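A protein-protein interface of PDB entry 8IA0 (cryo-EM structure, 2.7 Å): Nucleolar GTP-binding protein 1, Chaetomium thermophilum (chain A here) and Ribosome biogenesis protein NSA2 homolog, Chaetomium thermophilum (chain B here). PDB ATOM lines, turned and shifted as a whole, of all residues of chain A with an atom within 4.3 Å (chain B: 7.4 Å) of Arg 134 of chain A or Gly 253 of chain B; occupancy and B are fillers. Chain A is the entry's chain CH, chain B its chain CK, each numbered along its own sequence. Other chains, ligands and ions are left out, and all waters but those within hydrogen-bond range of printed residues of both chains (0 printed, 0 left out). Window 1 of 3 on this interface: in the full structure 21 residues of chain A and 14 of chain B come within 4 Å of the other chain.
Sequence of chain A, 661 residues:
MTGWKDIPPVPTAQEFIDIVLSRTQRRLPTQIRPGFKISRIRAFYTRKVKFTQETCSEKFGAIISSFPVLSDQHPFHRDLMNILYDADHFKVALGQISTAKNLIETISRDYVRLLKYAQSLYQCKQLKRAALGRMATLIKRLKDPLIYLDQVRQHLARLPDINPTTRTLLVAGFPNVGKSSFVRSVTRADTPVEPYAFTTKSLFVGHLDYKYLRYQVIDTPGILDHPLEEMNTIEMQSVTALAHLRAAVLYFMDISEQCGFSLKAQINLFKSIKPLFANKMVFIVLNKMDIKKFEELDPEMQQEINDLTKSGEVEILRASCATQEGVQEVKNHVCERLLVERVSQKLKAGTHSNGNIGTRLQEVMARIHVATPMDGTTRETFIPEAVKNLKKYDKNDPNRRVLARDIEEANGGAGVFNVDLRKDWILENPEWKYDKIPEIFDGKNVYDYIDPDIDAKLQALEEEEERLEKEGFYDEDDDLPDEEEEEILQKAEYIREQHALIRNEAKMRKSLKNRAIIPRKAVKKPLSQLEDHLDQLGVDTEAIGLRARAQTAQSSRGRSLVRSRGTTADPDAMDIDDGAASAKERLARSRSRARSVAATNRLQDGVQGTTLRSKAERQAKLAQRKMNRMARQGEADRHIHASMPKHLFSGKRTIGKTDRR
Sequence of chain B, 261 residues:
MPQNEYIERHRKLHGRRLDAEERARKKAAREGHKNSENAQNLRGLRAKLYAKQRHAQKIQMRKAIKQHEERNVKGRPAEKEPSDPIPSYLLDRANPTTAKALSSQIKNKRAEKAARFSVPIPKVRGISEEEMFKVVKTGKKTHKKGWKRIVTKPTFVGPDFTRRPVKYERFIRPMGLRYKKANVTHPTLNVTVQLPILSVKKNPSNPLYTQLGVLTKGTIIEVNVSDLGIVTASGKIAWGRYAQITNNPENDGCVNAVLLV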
ATOM      1  N   ILE A 107      -5.391 -21.373 -20.686  1.00  0.00           N
ATOM      2  CA  ILE A 107      -6.039 -20.378 -21.537  1.00  0.00           C
ATOM      3  C   ILE A 107      -5.546 -20.509 -22.971  1.00  0.00           C
ATOM      4  O   ILE A 107      -6.335 -20.451 -23.923  1.00  0.00           O
ATOM      5  CB  ILE A 107      -5.803 -18.962 -20.981  1.00  0.00           C
ATOM      6  CG1 ILE A 107      -6.707 -18.701 -19.778  1.00  0.00           C
ATOM      7  CG2 ILE A 107      -6.049 -17.915 -22.048  1.00  0.00           C
ATOM      8  CD1 ILE A 107      -6.413 -17.399 -19.076  1.00  0.00           C
ATOM      9  N   TYR A 111      -8.022 -21.519 -26.290  1.00  0.00           N
ATOM     10  CA  TYR A 111      -8.292 -20.627 -27.412  1.00  0.00           C
ATOM     11  C   TYR A 111      -7.679 -21.118 -28.716  1.00  0.00           C
ATOM     12  O   TYR A 111      -8.144 -20.720 -29.788  1.00  0.00           O
ATOM     13  CB  TYR A 111      -7.804 -19.219 -27.087  1.00  0.00           C
ATOM     14  CG  TYR A 111      -8.791 -18.435 -26.260  1.00  0.00           C
ATOM     15  CD1 TYR A 111      -9.774 -17.668 -26.861  1.00  0.00           C
ATOM     16  CD2 TYR A 111      -8.747 -18.472 -24.874  1.00  0.00           C
ATOM     17  CE1 TYR A 111     -10.680 -16.955 -26.109  1.00  0.00           C
ATOM     18  CE2 TYR A 111      -9.649 -17.763 -24.115  1.00  0.00           C
ATOM     19  CZ  TYR A 111     -10.612 -17.006 -24.737  1.00  0.00           C
ATOM     20  OH  TYR A 111     -11.515 -16.295 -23.983  1.00  0.00           O
ATOM     21  N   LEU A 114     -10.428 -23.189 -30.108  1.00  0.00           N
ATOM     22  CA  LEU A 114     -11.475 -22.342 -30.668  1.00  0.00           C
ATOM     23  C   LEU A 114     -11.066 -21.774 -32.021  1.00  0.00           C
ATOM     24  O   LEU A 114     -11.883 -21.707 -32.946  1.00  0.00           O
ATOM     25  CB  LEU A 114     -11.810 -21.212 -29.696  1.00  0.00           C
ATOM     26  CG  LEU A 114     -12.501 -21.608 -28.394  1.00  0.00           C
ATOM     27  CD1 LEU A 114     -12.729 -20.389 -27.519  1.00  0.00           C
ATOM     28  CD2 LEU A 114     -13.811 -22.315 -28.680  1.00  0.00           C
ATOM     29  N   ALA A 130      -9.239 -11.886 -26.925  1.00  0.00           N
ATOM     30  CA  ALA A 130      -9.744 -12.473 -25.689  1.00  0.00           C
ATOM     31  C   ALA A 130      -8.663 -13.283 -24.988  1.00  0.00           C
ATOM     32  O   ALA A 130      -8.507 -13.204 -23.765  1.00  0.00           O
ATOM     33  CB  ALA A 130     -10.967 -13.341 -25.983  1.00  0.00           C
ATOM     34  N   ALA A 131      -7.906 -14.073 -25.751  1.00  0.00           N
ATOM     35  CA  ALA A 131      -6.840 -14.873 -25.159  1.00  0.00           C
ATOM     36  C   ALA A 131      -5.767 -13.987 -24.540  1.00  0.00           C
ATOM     37  O   ALA A 131      -5.287 -14.253 -23.432  1.00  0.00           O
ATOM     38  CB  ALA A 131      -6.234 -15.800 -26.213  1.00  0.00           C
ATOM     39  N   LEU A 132      -5.381 -12.923 -25.245  1.00  0.00           N
ATOM     40  CA  LEU A 132      -4.346 -12.034 -24.729  1.00  0.00           C
ATOM     41  C   LEU A 132      -4.873 -11.180 -23.583  1.00  0.00           C
ATOM     42  O   LEU A 132      -4.142 -10.891 -22.629  1.00  0.00           O
ATOM     43  CB  LEU A 132      -3.806 -11.151 -25.853  1.00  0.00           C
ATOM     44  CG  LEU A 132      -2.549 -11.630 -26.581  1.00  0.00           C
ATOM     45  CD1 LEU A 132      -2.701 -13.057 -27.074  1.00  0.00           C
ATOM     46  CD2 LEU A 132      -2.224 -10.701 -27.733  1.00  0.00           C
ATOM     47  N   GLY A 133      -6.136 -10.763 -23.663  1.00  0.00           N
ATOM     48  CA  GLY A 133      -6.698  -9.934 -22.610  1.00  0.00           C
ATOM     49  C   GLY A 133      -6.827 -10.668 -21.291  1.00  0.00           C
ATOM     50  O   GLY A 133      -6.644 -10.082 -20.221  1.00  0.00           O
ATOM     51  N   ARG A 134      -7.149 -11.962 -21.346  1.00  0.00           N
ATOM     52  CA  ARG A 134      -7.261 -12.746 -20.121  1.00  0.00           C
ATOM     53  C   ARG A 134      -5.894 -13.009 -19.506  1.00  0.00           C
ATOM     54  O   ARG A 134      -5.750 -13.026 -18.279  1.00  0.00           O
ATOM     55  CB  ARG A 134      -7.992 -14.056 -20.407  1.00  0.00           C
ATOM     56  CG  ARG A 134      -9.428 -13.852 -20.829  1.00  0.00           C
ATOM     57  CD  ARG A 134     -10.109 -15.155 -21.184  1.00  0.00           C
ATOM     58  NE  ARG A 134     -10.049 -16.127 -20.101  1.00  0.00           N
ATOM     59  CZ  ARG A 134     -10.962 -17.063 -19.888  1.00  0.00           C
ATOM     60  NH1 ARG A 134     -12.039 -17.164 -20.648  1.00  0.00           N
ATOM     61  NH2 ARG A 134     -10.791 -17.921 -18.888  1.00  0.00           N
ATOM     62  N   MET A 135      -4.876 -13.223 -20.342  1.00  0.00           N
ATOM     63  CA  MET A 135      -3.521 -13.381 -19.826  1.00  0.00           C
ATOM     64  C   MET A 135      -3.042 -12.106 -19.147  1.00  0.00           C
ATOM     65  O   MET A 135      -2.340 -12.159 -18.131  1.00  0.00           O
ATOM     66  CB  MET A 135      -2.570 -13.787 -20.951  1.00  0.00           C
ATOM     67  CG  MET A 135      -2.835 -15.168 -21.521  1.00  0.00           C
ATOM     68  SD  MET A 135      -1.588 -15.686 -22.716  1.00  0.00           S
ATOM     69  CE  MET A 135      -2.605 -16.023 -24.148  1.00  0.00           C
ATOM     70  N   ALA A 136      -3.403 -10.947 -19.701  1.00  0.00           N
ATOM     71  CA  ALA A 136      -3.046  -9.681 -19.069  1.00  0.00           C
ATOM     72  C   ALA A 136      -3.743  -9.513 -17.724  1.00  0.00           C
ATOM     73  O   ALA A 136      -3.141  -9.019 -16.764  1.00  0.00           O
ATOM     74  CB  ALA A 136      -3.385  -8.517 -19.999  1.00  0.00           C
ATOM     75  N   THR A 137      -5.013  -9.912 -17.638  1.00  0.00           N
ATOM     76  CA  THR A 137      -5.763  -9.743 -16.396  1.00  0.00           C
ATOM     77  C   THR A 137      -5.172 -10.583 -15.270  1.00  0.00           C
ATOM     78  O   THR A 137      -5.126 -10.141 -14.116  1.00  0.00           O
ATOM     79  CB  THR A 137      -7.231 -10.102 -16.612  1.00  0.00           C
ATOM     80  OG1 THR A 137      -7.634  -9.704 -17.927  1.00  0.00           O
ATOM     81  CG2 THR A 137      -8.104  -9.398 -15.589  1.00  0.00           C
ATOM     82  N   LEU A 138      -4.730 -11.802 -15.582  1.00  0.00           N
ATOM     83  CA  LEU A 138      -4.155 -12.664 -14.554  1.00  0.00           C
ATOM     84  C   LEU A 138      -2.866 -12.077 -13.995  1.00  0.00           C
ATOM     85  O   LEU A 138      -2.604 -12.170 -12.790  1.00  0.00           O
ATOM     86  CB  LEU A 138      -3.909 -14.062 -15.118  1.00  0.00           C
ATOM     87  CG  LEU A 138      -5.104 -15.014 -15.084  1.00  0.00           C
ATOM     88  CD1 LEU A 138      -4.809 -16.276 -15.871  1.00  0.00           C
ATOM     89  CD2 LEU A 138      -5.479 -15.350 -13.649  1.00  0.00           C
ATOM     90  N   TYR B 179     -19.281 -26.071 -23.705  1.00  0.00           N
ATOM     91  CA  TYR B 179     -19.211 -25.367 -22.435  1.00  0.00           C
ATOM     92  C   TYR B 179     -20.191 -25.982 -21.448  1.00  0.00           C
ATOM     93  O   TYR B 179     -21.269 -26.453 -21.817  1.00  0.00           O
ATOM     94  CB  TYR B 179     -19.499 -23.868 -22.594  1.00  0.00           C
ATOM     95  CG  TYR B 179     -18.617 -23.181 -23.604  1.00  0.00           C
ATOM     96  CD1 TYR B 179     -18.937 -23.180 -24.952  1.00  0.00           C
ATOM     97  CD2 TYR B 179     -17.460 -22.528 -23.207  1.00  0.00           C
ATOM     98  CE1 TYR B 179     -18.124 -22.554 -25.873  1.00  0.00           C
ATOM     99  CE2 TYR B 179     -16.647 -21.899 -24.119  1.00  0.00           C
ATOM    100  CZ  TYR B 179     -16.983 -21.912 -25.451  1.00  0.00           C
ATOM    101  OH  TYR B 179     -16.174 -21.285 -26.368  1.00  0.00           O
ATOM    102  N   ASN B 183     -20.700 -17.527 -16.385  1.00  0.00           N
ATOM    103  CA  ASN B 183     -20.634 -16.434 -15.419  1.00  0.00           C
ATOM    104  C   ASN B 183     -21.999 -15.761 -15.380  1.00  0.00           C
ATOM    105  O   ASN B 183     -22.337 -14.965 -16.257  1.00  0.00           O
ATOM    106  CB  ASN B 183     -19.535 -15.448 -15.800  1.00  0.00           C
ATOM    107  CG  ASN B 183     -18.258 -16.136 -16.231  1.00  0.00           C
ATOM    108  OD1 ASN B 183     -17.782 -17.057 -15.568  1.00  0.00           O
ATOM    109  ND2 ASN B 183     -17.695 -15.693 -17.346  1.00  0.00           N
ATOM    110  N   ASN B 247     -23.692 -12.149 -24.094  1.00  0.00           N
ATOM    111  CA  ASN B 247     -22.463 -11.950 -24.846  1.00  0.00           C
ATOM    112  C   ASN B 247     -22.486 -12.804 -26.112  1.00  0.00           C
ATOM    113  O   ASN B 247     -23.501 -13.410 -26.462  1.00  0.00           O
ATOM    114  CB  ASN B 247     -21.246 -12.270 -23.977  1.00  0.00           C
ATOM    115  CG  ASN B 247     -21.029 -13.757 -23.805  1.00  0.00           C
ATOM    116  OD1 ASN B 247     -21.931 -14.483 -23.392  1.00  0.00           O
ATOM    117  ND2 ASN B 247     -19.829 -14.220 -24.126  1.00  0.00           N
ATOM    118  N   ASN B 248     -21.343 -12.853 -26.797  1.00  0.00           N
ATOM    119  CA  ASN B 248     -21.161 -13.653 -28.006  1.00  0.00           C
ATOM    120  C   ASN B 248     -20.133 -14.733 -27.699  1.00  0.00           C
ATOM    121  O   ASN B 248     -18.920 -14.499 -27.813  1.00  0.00           O
ATOM    122  CB  ASN B 248     -20.717 -12.785 -29.180  1.00  0.00           C
ATOM    123  CG  ASN B 248     -21.870 -12.060 -29.837  1.00  0.00           C
ATOM    124  OD1 ASN B 248     -22.894 -12.661 -30.158  1.00  0.00           O
ATOM    125  ND2 ASN B 248     -21.710 -10.759 -30.040  1.00  0.00           N
ATOM    126  N   PRO B 249     -20.572 -15.930 -27.304  1.00  0.00           N
ATOM    127  CA  PRO B 249     -19.604 -16.969 -26.917  1.00  0.00           C
ATOM    128  C   PRO B 249     -18.684 -17.403 -28.043  1.00  0.00           C
ATOM    129  O   PRO B 249     -17.615 -17.965 -27.779  1.00  0.00           O
ATOM    130  CB  PRO B 249     -20.503 -18.119 -26.441  1.00  0.00           C
ATOM    131  CG  PRO B 249     -21.787 -17.471 -26.067  1.00  0.00           C
ATOM    132  CD  PRO B 249     -21.958 -16.325 -27.011  1.00  0.00           C
ATOM    133  N   GLU B 250     -19.072 -17.172 -29.298  1.00  0.00           N
ATOM    134  CA  GLU B 250     -18.205 -17.546 -30.411  1.00  0.00           C
ATOM    135  C   GLU B 250     -17.021 -16.595 -30.532  1.00  0.00           C
ATOM    136  O   GLU B 250     -15.909 -17.017 -30.871  1.00  0.00           O
ATOM    137  CB  GLU B 250     -18.996 -17.590 -31.722  1.00  0.00           C
ATOM    138  CG  GLU B 250     -19.914 -16.402 -31.985  1.00  0.00           C
ATOM    139  CD  GLU B 250     -21.202 -16.452 -31.187  1.00  0.00           C
ATOM    140  OE1 GLU B 250     -21.580 -17.554 -30.734  1.00  0.00           O
ATOM    141  OE2 GLU B 250     -21.838 -15.391 -31.012  1.00  0.00           O
ATOM    142  N   ASN B 251     -17.238 -15.306 -30.263  1.00  0.00           N
ATOM    143  CA  ASN B 251     -16.150 -14.338 -30.346  1.00  0.00           C
ATOM    144  C   ASN B 251     -15.373 -14.253 -29.038  1.00  0.00           C
ATOM    145  O   ASN B 251     -14.144 -14.131 -29.051  1.00  0.00           O
ATOM    146  CB  ASN B 251     -16.698 -12.963 -30.725  1.00  0.00           C
ATOM    147  CG  ASN B 251     -17.571 -13.005 -31.958  1.00  0.00           C
ATOM    148  OD1 ASN B 251     -18.779 -12.787 -31.884  1.00  0.00           O
ATOM    149  ND2 ASN B 251     -16.965 -13.285 -33.102  1.00  0.00           N
ATOM    150  N   ASP B 252     -16.068 -14.316 -27.907  1.00  0.00           N
ATOM    151  CA  ASP B 252     -15.457 -14.277 -26.580  1.00  0.00           C
ATOM    152  C   ASP B 252     -15.538 -15.695 -26.026  1.00  0.00           C
ATOM    153  O   ASP B 252     -16.630 -16.242 -25.860  1.00  0.00           O
ATOM    154  CB  ASP B 252     -16.167 -13.276 -25.684  1.00  0.00           C
ATOM    155  CG  ASP B 252     -16.426 -11.958 -26.381  1.00  0.00           C
ATOM    156  OD1 ASP B 252     -15.489 -11.421 -27.009  1.00  0.00           O
ATOM    157  OD2 ASP B 252     -17.569 -11.461 -26.308  1.00  0.00           O
ATOM    158  N   GLY B 253     -14.386 -16.284 -25.722  1.00  0.00           N
ATOM    159  CA  GLY B 253     -14.347 -17.690 -25.369  1.00  0.00           C
ATOM    160  C   GLY B 253     -14.930 -18.019 -24.012  1.00  0.00           C
ATOM    161  O   GLY B 253     -14.262 -18.630 -23.173  1.00  0.00           O
ATOM    162  N   CYS B 254     -16.185 -17.630 -23.792  1.00  0.00           N
ATOM    163  CA  CYS B 254     -16.873 -17.865 -22.532  1.00  0.00           C
ATOM    164  C   CYS B 254     -18.342 -17.516 -22.704  1.00  0.00           C
ATOM    165  O   CYS B 254     -18.750 -16.942 -23.716  1.00  0.00           O
ATOM    166  CB  CYS B 254     -16.261 -17.048 -21.386  1.00  0.00           C
ATOM    167  SG  CYS B 254     -16.588 -15.276 -21.467  1.00  0.00           S
ATOM    168  N   VAL B 255     -19.138 -17.871 -21.699  1.00  0.00           N
ATOM    169  CA  VAL B 255     -20.571 -17.602 -21.684  1.00  0.00           C
ATOM    170  C   VAL B 255     -20.870 -16.689 -20.504  1.00  0.00           C
ATOM    171  O   VAL B 255     -20.528 -17.009 -19.359  1.00  0.00           O
ATOM    172  CB  VAL B 255     -21.391 -18.897 -21.598  1.00  0.00           C
ATOM    173  CG1 VAL B 255     -22.870 -18.579 -21.490  1.00  0.00           C
ATOM    174  CG2 VAL B 255     -21.121 -19.776 -22.802  1.00  0.00           C
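Of the 11 printed residues of chain B, 2 touch a printed residue of chain A. Along chain B the printed residues that touch a printed residue of chain A span positions 179 to 253. Along chain A the printed residues that touch a printed residue of chain B span positions 111 to 134. Among the printed residues, 4 pairs touch across the chains. Among the printed residues, no Asp or Glu carboxylate lies within 4 Å of a Lys or Arg side-chain nitrogen of the other chain.
N of Gly 253 of chain B lies within hydrogen-bond range of OH of Tyr 111 of chain A (3.4 Å).
The side-chain hydroxyl of Tyr 111 of chain A sits close to the guanidinium group of Arg 134 of chain A (3.5 Å).
Printed residues of chain B within 4 Å of Tyr 111 of chain A: Gly 253 (3.4 Å). Printed residues of chain B within 4 Å of Leu 114 of chain A: Tyr 179 (3.5 Å) and Gly 253 (3.8 Å). No residue of chain B comes within 4 Å of Gly 133 of chain A. Arg 134 of chain A touches just one residue of chain B: Gly 253 (3.7 Å). Printed residues of chain A within 4 Å of Tyr 179 of chain B: Leu 114 (3.5 Å). Of chain A, only Tyr 111, Leu 114 and Arg 134 come within 4 Å of Gly 253 of chain B. The nearest residue of chain B that does not touch Arg 134 of chain A is Cys 254 of chain B (4.3 Å). The nearest printed residue of chain A that does not touch Gly 253 of chain B is Ala 130 of chain A (4.5 Å). The nearest printed residue of chain A that does not touch Tyr 179 of chain B is Tyr 111 of chain A (7.0 Å).
Among the printed residues, pairs that only touch across the chains: Leu 114 of chain A with Tyr 179 of chain B (3.5 Å), Leu 114 of chain A with Gly 253 of chain B (3.8 Å) and Arg 134 of chain A with Gly 253 of chain B (3.7 Å).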
